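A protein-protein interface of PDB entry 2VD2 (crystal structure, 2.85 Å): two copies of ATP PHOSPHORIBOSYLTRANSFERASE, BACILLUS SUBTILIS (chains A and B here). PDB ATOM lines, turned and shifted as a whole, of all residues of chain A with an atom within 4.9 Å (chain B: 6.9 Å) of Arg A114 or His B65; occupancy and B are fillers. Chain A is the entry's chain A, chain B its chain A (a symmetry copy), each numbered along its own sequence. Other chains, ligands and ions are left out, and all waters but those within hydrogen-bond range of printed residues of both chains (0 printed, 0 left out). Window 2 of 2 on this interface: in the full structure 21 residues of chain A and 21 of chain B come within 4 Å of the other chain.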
ATOM      1  N   TRP A 108     -28.480  -1.387 -15.873  1.00  0.00           N
ATOM      2  CA  TRP A 108     -27.855  -1.596 -14.560  1.00  0.00           C
ATOM      3  C   TRP A 108     -26.645  -2.519 -14.593  1.00  0.00           C
ATOM      4  O   TRP A 108     -26.543  -3.410 -15.442  1.00  0.00           O
ATOM      5  CB  TRP A 108     -28.852  -2.227 -13.608  1.00  0.00           C
ATOM      6  CG  TRP A 108     -29.690  -1.263 -12.928  1.00  0.00           C
ATOM      7  CD1 TRP A 108     -31.006  -1.006 -13.174  1.00  0.00           C
ATOM      8  CD2 TRP A 108     -29.297  -0.401 -11.852  1.00  0.00           C
ATOM      9  NE1 TRP A 108     -31.459  -0.029 -12.313  1.00  0.00           N
ATOM     10  CE2 TRP A 108     -30.430   0.355 -11.492  1.00  0.00           C
ATOM     11  CE3 TRP A 108     -28.099  -0.195 -11.159  1.00  0.00           C
ATOM     12  CZ2 TRP A 108     -30.403   1.291 -10.469  1.00  0.00           C
ATOM     13  CZ3 TRP A 108     -28.076   0.743 -10.141  1.00  0.00           C
ATOM     14  CH2 TRP A 108     -29.222   1.468  -9.808  1.00  0.00           C
ATOM     15  N   ALA A 112     -22.504  -5.244  -8.237  1.00  0.00           N
ATOM     16  CA  ALA A 112     -22.358  -3.960  -7.563  1.00  0.00           C
ATOM     17  C   ALA A 112     -23.054  -2.855  -8.314  1.00  0.00           C
ATOM     18  O   ALA A 112     -22.442  -1.828  -8.601  1.00  0.00           O
ATOM     19  CB  ALA A 112     -20.897  -3.618  -7.427  1.00  0.00           C
ATOM     20  N   PRO A 113     -24.328  -3.068  -8.665  1.00  0.00           N
ATOM     21  CA  PRO A 113     -25.056  -1.931  -9.185  1.00  0.00           C
ATOM     22  C   PRO A 113     -24.983  -0.817  -8.153  1.00  0.00           C
ATOM     23  O   PRO A 113     -25.115  -1.069  -6.947  1.00  0.00           O
ATOM     24  CB  PRO A 113     -26.481  -2.459  -9.365  1.00  0.00           C
ATOM     25  CG  PRO A 113     -26.543  -3.710  -8.578  1.00  0.00           C
ATOM     26  CD  PRO A 113     -25.167  -4.272  -8.605  1.00  0.00           C
ATOM     27  N   ARG A 114     -24.776   0.399  -8.640  1.00  0.00           N
ATOM     28  CA  ARG A 114     -24.284   1.486  -7.817  1.00  0.00           C
ATOM     29  C   ARG A 114     -25.008   2.783  -8.165  1.00  0.00           C
ATOM     30  O   ARG A 114     -25.474   2.952  -9.305  1.00  0.00           O
ATOM     31  CB  ARG A 114     -22.772   1.619  -8.034  1.00  0.00           C
ATOM     32  CG  ARG A 114     -22.320   1.316  -9.491  1.00  0.00           C
ATOM     33  CD  ARG A 114     -20.812   1.075  -9.647  1.00  0.00           C
ATOM     34  NE  ARG A 114     -20.031   1.501  -8.479  1.00  0.00           N
ATOM     35  CZ  ARG A 114     -18.718   1.301  -8.343  1.00  0.00           C
ATOM     36  NH1 ARG A 114     -18.018   0.696  -9.311  1.00  0.00           N
ATOM     37  NH2 ARG A 114     -18.094   1.728  -7.245  1.00  0.00           N
ATOM     38  N   ILE A 115     -25.128   3.671  -7.173  1.00  0.00           N
ATOM     39  CA  ILE A 115     -25.707   4.999  -7.375  1.00  0.00           C
ATOM     40  C   ILE A 115     -24.808   6.089  -6.832  1.00  0.00           C
ATOM     41  O   ILE A 115     -24.347   6.035  -5.685  1.00  0.00           O
ATOM     42  CB  ILE A 115     -27.094   5.166  -6.710  1.00  0.00           C
ATOM     43  CG1 ILE A 115     -28.164   4.406  -7.492  1.00  0.00           C
ATOM     44  CG2 ILE A 115     -27.488   6.637  -6.627  1.00  0.00           C
ATOM     45  CD1 ILE A 115     -28.319   2.978  -7.044  1.00  0.00           C
ATOM     46  N   ALA A 116     -24.549   7.081  -7.671  1.00  0.00           N
ATOM     47  CA  ALA A 116     -24.032   8.339  -7.190  1.00  0.00           C
ATOM     48  C   ALA A 116     -25.245   9.200  -6.885  1.00  0.00           C
ATOM     49  O   ALA A 116     -26.197   9.223  -7.656  1.00  0.00           O
ATOM     50  CB  ALA A 116     -23.166   8.994  -8.230  1.00  0.00           C
ATOM     51  N   VAL A 134     -28.113  -2.407  -3.420  1.00  0.00           N
ATOM     52  CA  VAL A 134     -27.466  -1.418  -4.273  1.00  0.00           C
ATOM     53  C   VAL A 134     -26.311  -0.803  -3.489  1.00  0.00           C
ATOM     54  O   VAL A 134     -26.068  -1.165  -2.331  1.00  0.00           O
ATOM     55  CB  VAL A 134     -28.475  -0.324  -4.713  1.00  0.00           C
ATOM     56  CG1 VAL A 134     -28.477   0.846  -3.745  1.00  0.00           C
ATOM     57  CG2 VAL A 134     -28.167   0.140  -6.099  1.00  0.00           C
ATOM     58  N   GLU A 135     -25.610   0.136  -4.113  1.00  0.00           N
ATOM     59  CA  GLU A 135     -24.355   0.636  -3.586  1.00  0.00           C
ATOM     60  C   GLU A 135     -24.311   2.138  -3.791  1.00  0.00           C
ATOM     61  O   GLU A 135     -24.045   2.621  -4.885  1.00  0.00           O
ATOM     62  CB  GLU A 135     -23.229  -0.059  -4.328  1.00  0.00           C
ATOM     63  CG  GLU A 135     -21.832   0.286  -3.894  1.00  0.00           C
ATOM     64  CD  GLU A 135     -20.804  -0.433  -4.755  1.00  0.00           C
ATOM     65  OE1 GLU A 135     -21.098  -1.580  -5.205  1.00  0.00           O
ATOM     66  OE2 GLU A 135     -19.714   0.153  -4.998  1.00  0.00           O
ATOM     67  N   ILE A 137     -23.371   6.145  -3.209  1.00  0.00           N
ATOM     68  CA  ILE A 137     -22.164   6.896  -3.060  1.00  0.00           C
ATOM     69  C   ILE A 137     -22.583   8.340  -2.960  1.00  0.00           C
ATOM     70  O   ILE A 137     -23.171   8.885  -3.884  1.00  0.00           O
ATOM     71  CB  ILE A 137     -21.238   6.661  -4.255  1.00  0.00           C
ATOM     72  CG1 ILE A 137     -21.219   5.172  -4.640  1.00  0.00           C
ATOM     73  CG2 ILE A 137     -19.847   7.129  -3.921  1.00  0.00           C
ATOM     74  CD1 ILE A 137     -20.383   4.839  -5.877  1.00  0.00           C
ATOM     75  N   GLY A 150     -18.429   6.334 -14.903  1.00  0.00           N
ATOM     76  CA  GLY A 150     -18.779   5.049 -14.330  1.00  0.00           C
ATOM     77  C   GLY A 150     -18.592   4.921 -12.836  1.00  0.00           C
ATOM     78  O   GLY A 150     -18.560   3.813 -12.305  1.00  0.00           O
ATOM     79  N   LEU A 151     -18.491   6.037 -12.135  1.00  0.00           N
ATOM     80  CA  LEU A 151     -18.478   5.943 -10.701  1.00  0.00           C
ATOM     81  C   LEU A 151     -19.627   5.045 -10.350  1.00  0.00           C
ATOM     82  O   LEU A 151     -19.527   4.139  -9.530  1.00  0.00           O
ATOM     83  CB  LEU A 151     -18.686   7.297 -10.045  1.00  0.00           C
ATOM     84  CG  LEU A 151     -18.661   7.156  -8.529  1.00  0.00           C
ATOM     85  CD1 LEU A 151     -17.418   6.399  -8.072  1.00  0.00           C
ATOM     86  CD2 LEU A 151     -18.731   8.514  -7.876  1.00  0.00           C
ATOM     87  N   ALA A 152     -20.735   5.338 -10.990  1.00  0.00           N
ATOM     88  CA  ALA A 152     -21.923   4.608 -10.771  1.00  0.00           C
ATOM     89  C   ALA A 152     -22.715   4.780 -12.027  1.00  0.00           C
ATOM     90  O   ALA A 152     -22.742   5.855 -12.621  1.00  0.00           O
ATOM     91  CB  ALA A 152     -22.654   5.162  -9.610  1.00  0.00           C
ATOM     92  N   ASP A 153     -23.353   3.701 -12.438  1.00  0.00           N
ATOM     93  CA  ASP A 153     -24.112   3.693 -13.669  1.00  0.00           C
ATOM     94  C   ASP A 153     -25.424   4.471 -13.520  1.00  0.00           C
ATOM     95  O   ASP A 153     -26.080   4.785 -14.510  1.00  0.00           O
ATOM     96  CB  ASP A 153     -24.372   2.246 -14.140  1.00  0.00           C
ATOM     97  CG  ASP A 153     -23.832   1.175 -13.159  1.00  0.00           C
ATOM     98  OD1 ASP A 153     -23.072   0.297 -13.636  1.00  0.00           O
ATOM     99  OD2 ASP A 153     -24.160   1.211 -11.935  1.00  0.00           O
ATOM    100  N   ARG A 154     -25.793   4.791 -12.283  1.00  0.00           N
ATOM    101  CA  ARG A 154     -27.090   5.380 -11.985  1.00  0.00           C
ATOM    102  C   ARG A 154     -26.952   6.425 -10.896  1.00  0.00           C
ATOM    103  O   ARG A 154     -26.417   6.143  -9.826  1.00  0.00           O
ATOM    104  CB  ARG A 154     -28.026   4.293 -11.487  1.00  0.00           C
ATOM    105  CG  ARG A 154     -28.400   3.288 -12.544  1.00  0.00           C
ATOM    106  CD  ARG A 154     -29.418   3.869 -13.497  1.00  0.00           C
ATOM    107  NE  ARG A 154     -30.074   2.811 -14.263  1.00  0.00           N
ATOM    108  CZ  ARG A 154     -29.685   2.378 -15.461  1.00  0.00           C
ATOM    109  NH1 ARG A 154     -28.635   2.909 -16.077  1.00  0.00           N
ATOM    110  NH2 ARG A 154     -30.367   1.405 -16.049  1.00  0.00           N
ATOM    111  N   THR B  60     -11.748  12.674  -3.512  1.00  0.00           N
ATOM    112  CA  THR B  60     -11.377  11.371  -3.008  1.00  0.00           C
ATOM    113  C   THR B  60     -12.383  10.348  -3.522  1.00  0.00           C
ATOM    114  O   THR B  60     -12.001   9.395  -4.206  1.00  0.00           O
ATOM    115  CB  THR B  60     -11.259  11.337  -1.512  1.00  0.00           C
ATOM    116  OG1 THR B  60     -10.254  12.274  -1.107  1.00  0.00           O
ATOM    117  CG2 THR B  60     -10.884   9.938  -1.034  1.00  0.00           C
ATOM    118  N   THR B  61     -13.671  10.555  -3.264  1.00  0.00           N
ATOM    119  CA  THR B  61     -14.664   9.615  -3.798  1.00  0.00           C
ATOM    120  C   THR B  61     -14.141   8.979  -5.093  1.00  0.00           C
ATOM    121  O   THR B  61     -13.792   7.792  -5.135  1.00  0.00           O
ATOM    122  CB  THR B  61     -15.981  10.293  -4.111  1.00  0.00           C
ATOM    123  OG1 THR B  61     -16.317  11.183  -3.045  1.00  0.00           O
ATOM    124  CG2 THR B  61     -17.051   9.267  -4.293  1.00  0.00           C
ATOM    125  N   TYR B  62     -14.027   9.789  -6.135  1.00  0.00           N
ATOM    126  CA  TYR B  62     -13.691   9.245  -7.414  1.00  0.00           C
ATOM    127  C   TYR B  62     -12.445   8.402  -7.263  1.00  0.00           C
ATOM    128  O   TYR B  62     -12.419   7.223  -7.645  1.00  0.00           O
ATOM    129  CB  TYR B  62     -13.487  10.357  -8.421  1.00  0.00           C
ATOM    130  CG  TYR B  62     -14.782  11.020  -8.827  1.00  0.00           C
ATOM    131  CD1 TYR B  62     -15.707  10.358  -9.626  1.00  0.00           C
ATOM    132  CD2 TYR B  62     -15.077  12.313  -8.421  1.00  0.00           C
ATOM    133  CE1 TYR B  62     -16.899  10.968 -10.012  1.00  0.00           C
ATOM    134  CE2 TYR B  62     -16.265  12.936  -8.807  1.00  0.00           C
ATOM    135  CZ  TYR B  62     -17.178  12.260  -9.599  1.00  0.00           C
ATOM    136  OH  TYR B  62     -18.371  12.885  -9.954  1.00  0.00           O
ATOM    137  N   VAL B  63     -11.418   8.997  -6.676  1.00  0.00           N
ATOM    138  CA  VAL B  63     -10.161   8.293  -6.475  1.00  0.00           C
ATOM    139  C   VAL B  63     -10.390   7.011  -5.683  1.00  0.00           C
ATOM    140  O   VAL B  63      -9.894   5.979  -6.067  1.00  0.00           O
ATOM    141  CB  VAL B  63      -9.107   9.199  -5.817  1.00  0.00           C
ATOM    142  CG1 VAL B  63      -8.002   8.384  -5.209  1.00  0.00           C
ATOM    143  CG2 VAL B  63      -8.566  10.162  -6.835  1.00  0.00           C
ATOM    144  N   GLU B  64     -11.194   7.062  -4.627  1.00  0.00           N
ATOM    145  CA  GLU B  64     -11.489   5.869  -3.797  1.00  0.00           C
ATOM    146  C   GLU B  64     -12.059   4.688  -4.608  1.00  0.00           C
ATOM    147  O   GLU B  64     -11.773   3.521  -4.323  1.00  0.00           O
ATOM    148  CB  GLU B  64     -12.456   6.242  -2.662  1.00  0.00           C
ATOM    149  CG  GLU B  64     -12.630   5.190  -1.566  1.00  0.00           C
ATOM    150  CD  GLU B  64     -13.560   5.677  -0.438  1.00  0.00           C
ATOM    151  OE1 GLU B  64     -13.741   6.908  -0.305  1.00  0.00           O
ATOM    152  OE2 GLU B  64     -14.128   4.845   0.318  1.00  0.00           O
ATOM    153  N   HIS B  65     -12.849   5.011  -5.625  1.00  0.00           N
ATOM    154  CA  HIS B  65     -13.440   4.008  -6.497  1.00  0.00           C
ATOM    155  C   HIS B  65     -12.584   3.714  -7.733  1.00  0.00           C
ATOM    156  O   HIS B  65     -12.877   2.803  -8.496  1.00  0.00           O
ATOM    157  CB  HIS B  65     -14.840   4.462  -6.885  1.00  0.00           C
ATOM    158  CG  HIS B  65     -15.765   4.573  -5.710  1.00  0.00           C
ATOM    159  ND1 HIS B  65     -15.824   5.697  -4.915  1.00  0.00           N
ATOM    160  CD2 HIS B  65     -16.636   3.685  -5.171  1.00  0.00           C
ATOM    161  CE1 HIS B  65     -16.703   5.502  -3.946  1.00  0.00           C
ATOM    162  NE2 HIS B  65     -17.207   4.289  -4.079  1.00  0.00           N
ATOM    163  N   GLY B  66     -11.510   4.476  -7.923  1.00  0.00           N
ATOM    164  CA  GLY B  66     -10.600   4.254  -9.041  1.00  0.00           C
ATOM    165  C   GLY B  66     -11.237   4.709 -10.332  1.00  0.00           C
ATOM    166  O   GLY B  66     -10.771   4.362 -11.426  1.00  0.00           O
ATOM    167  N   VAL B  67     -12.320   5.471 -10.212  1.00  0.00           N
ATOM    168  CA  VAL B  67     -12.874   6.149 -11.350  1.00  0.00           C
ATOM    169  C   VAL B  67     -11.796   7.149 -11.769  1.00  0.00           C
ATOM    170  O   VAL B  67     -11.535   7.333 -12.965  1.00  0.00           O
ATOM    171  CB  VAL B  67     -14.217   6.778 -10.996  1.00  0.00           C
ATOM    172  CG1 VAL B  67     -14.586   7.893 -11.959  1.00  0.00           C
ATOM    173  CG2 VAL B  67     -15.270   5.685 -10.987  1.00  0.00           C
ATOM    174  N   ALA B  68     -11.143   7.754 -10.783  1.00  0.00           N
ATOM    175  CA  ALA B  68      -9.874   8.435 -11.017  1.00  0.00           C
ATOM    176  C   ALA B  68      -8.794   7.630 -10.306  1.00  0.00           C
ATOM    177  O   ALA B  68      -8.980   7.183  -9.169  1.00  0.00           O
ATOM    178  CB  ALA B  68      -9.908   9.831 -10.492  1.00  0.00           C
ATOM    179  N   ARG B  83     -10.566   7.168   5.603  1.00  0.00           N
ATOM    180  CA  ARG B  83     -10.986   6.455   4.381  1.00  0.00           C
ATOM    181  C   ARG B  83      -9.799   5.954   3.526  1.00  0.00           C
ATOM    182  O   ARG B  83      -8.650   6.326   3.777  1.00  0.00           O
ATOM    183  CB  ARG B  83     -11.847   7.381   3.525  1.00  0.00           C
ATOM    184  CG  ARG B  83     -11.052   8.496   2.829  1.00  0.00           C
ATOM    185  CD  ARG B  83     -11.958   9.599   2.310  1.00  0.00           C
ATOM    186  NE  ARG B  83     -13.161   9.073   1.652  1.00  0.00           N
ATOM    187  CZ  ARG B  83     -13.909   9.743   0.772  1.00  0.00           C
ATOM    188  NH1 ARG B  83     -14.992   9.165   0.248  1.00  0.00           N
ATOM    189  NH2 ARG B  83     -13.595  10.988   0.411  1.00  0.00           N
ATOM    190  N   ASP B  84     -10.106   5.144   2.503  1.00  0.00           N
ATOM    191  CA  ASP B  84      -9.081   4.426   1.715  1.00  0.00           C
ATOM    192  C   ASP B  84      -8.563   5.179   0.497  1.00  0.00           C
ATOM    193  O   ASP B  84      -9.253   5.329  -0.503  1.00  0.00           O
ATOM    194  CB  ASP B  84      -9.587   3.054   1.239  1.00  0.00           C
ATOM    195  CG  ASP B  84      -8.608   2.369   0.261  1.00  0.00           C
ATOM    196  OD1 ASP B  84      -8.155   3.022  -0.717  1.00  0.00           O
ATOM    197  OD2 ASP B  84      -8.293   1.175   0.474  1.00  0.00           O
ATOM    198  N   VAL B  85      -7.324   5.621   0.596  1.00  0.00           N
ATOM    199  CA  VAL B  85      -6.538   6.100  -0.535  1.00  0.00           C
ATOM    200  C   VAL B  85      -5.181   6.285   0.076  1.00  0.00           C
ATOM    201  O   VAL B  85      -5.073   6.672   1.246  1.00  0.00           O
ATOM    202  CB  VAL B  85      -6.985   7.468  -1.108  1.00  0.00           C
ATOM    203  CG1 VAL B  85      -8.065   7.297  -2.165  1.00  0.00           C
ATOM    204  CG2 VAL B  85      -7.449   8.404   0.007  1.00  0.00           C
ATOM    205  N   ASN B 186      -5.393   5.870  -5.799  1.00  0.00           N
ATOM    206  CA  ASN B 186      -6.244   4.723  -5.592  1.00  0.00           C
ATOM    207  C   ASN B 186      -5.312   3.521  -5.552  1.00  0.00           C
ATOM    208  O   ASN B 186      -4.441   3.391  -6.407  1.00  0.00           O
ATOM    209  CB  ASN B 186      -7.239   4.631  -6.732  1.00  0.00           C
ATOM    210  CG  ASN B 186      -7.986   3.354  -6.730  1.00  0.00           C
ATOM    211  OD1 ASN B 186      -7.391   2.285  -6.827  1.00  0.00           O
ATOM    212  ND2 ASN B 186      -9.297   3.435  -6.608  1.00  0.00           N
ATOM    213  N   SER B 189      -5.530   1.154  -8.436  1.00  0.00           N
ATOM    214  CA  SER B 189      -5.037   1.894  -9.582  1.00  0.00           C
ATOM    215  C   SER B 189      -3.518   1.881  -9.530  1.00  0.00           C
ATOM    216  O   SER B 189      -2.857   1.510 -10.503  1.00  0.00           O
ATOM    217  CB  SER B 189      -5.575   3.328  -9.588  1.00  0.00           C
ATOM    218  OG  SER B 189      -6.998   3.349  -9.487  1.00  0.00           O
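Among the printed residues, merely in contact across the chains: Arg A114 with His B65 (3.2 Å), Ile A137 with Thr B61 (3.5 Å), Ile A137 with His B65 (3.5 Å), Gly A150 with Val B67 (3.9 Å), Leu A151 with Tyr B62 (3.7 Å), Leu A151 with His B65 (3.4 Å) and Leu A151 with Val B67 (3.2 Å).
No position is printed for both chains.
Of the 7 pairs that touch across the chains among the printed residues, none has its exchanged pair printed and touching as well.
Of the 14 printed residues of chain A, 4 touch a printed residue of chain B.
Hydrophobic or aromatic side chains of chain A within 4 Å of the printed part of chain B: Ile A137 and Leu A151.
Along chain A the printed residues that touch a printed residue of chain B span positions 114 to 151.
Of the 14 printed residues of chain B, 4 touch a printed residue of chain A.
Among the printed residues, 7 pairs touch across the chains.
Among the printed residues, no Asp or Glu carboxylate lies within 4 Å of a Lys or Arg side-chain nitrogen of the other chain.
Of chain B, only His B65 comes within 4 Å of Arg A114.
Of the printed residues of chain B, Gly A150 touches Val B67.
Of the printed residues of chain B, Leu A151 touches Tyr B62 (3.7 Å), His B65 (3.4 Å) and Val B67 (3.2 Å).
Asp A153 touches none of the printed residues of chain B.
Of chain A, only Arg A114, Ile A137 and Leu A151 come within 4 Å of His B65.
Of the printed residues of chain A, Val B67 touches Gly A150 (3.9 Å) and Leu A151 (3.2 Å).
The nearest residue of chain B that does not touch Arg A114 is Val B67 (5.9 Å).
The nearest residue of chain A that does not touch His B65 is Glu A135 (4.7 Å).
The backbone carbonyl oxygen of Leu A151 lies within hydrogen-bond range of the guanidinium group of Arg A114, 2.9 Å away.
The backbone carbonyl oxygen (O) of Thr B61 lies within hydrogen-bond range of a ring nitrogen (ND1) of His B65 (2.9 Å).
The guanidinium group of Arg A114 is in salt-bridge range of the side-chain carboxylate of Glu A135 (3.2 Å).
N of Arg A114 lies close to OD2 of Asp A153 (3.4 Å).
The backbone carbonyl oxygen (O) of Tyr B62 lies within hydrogen-bond range of the backbone NH (N) of Ala B68.
The backbone carbonyl oxygen (O) of Ile A115 lies within hydrogen-bond range of the backbone NH (N) of Ile A137, at 2.7 Å.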
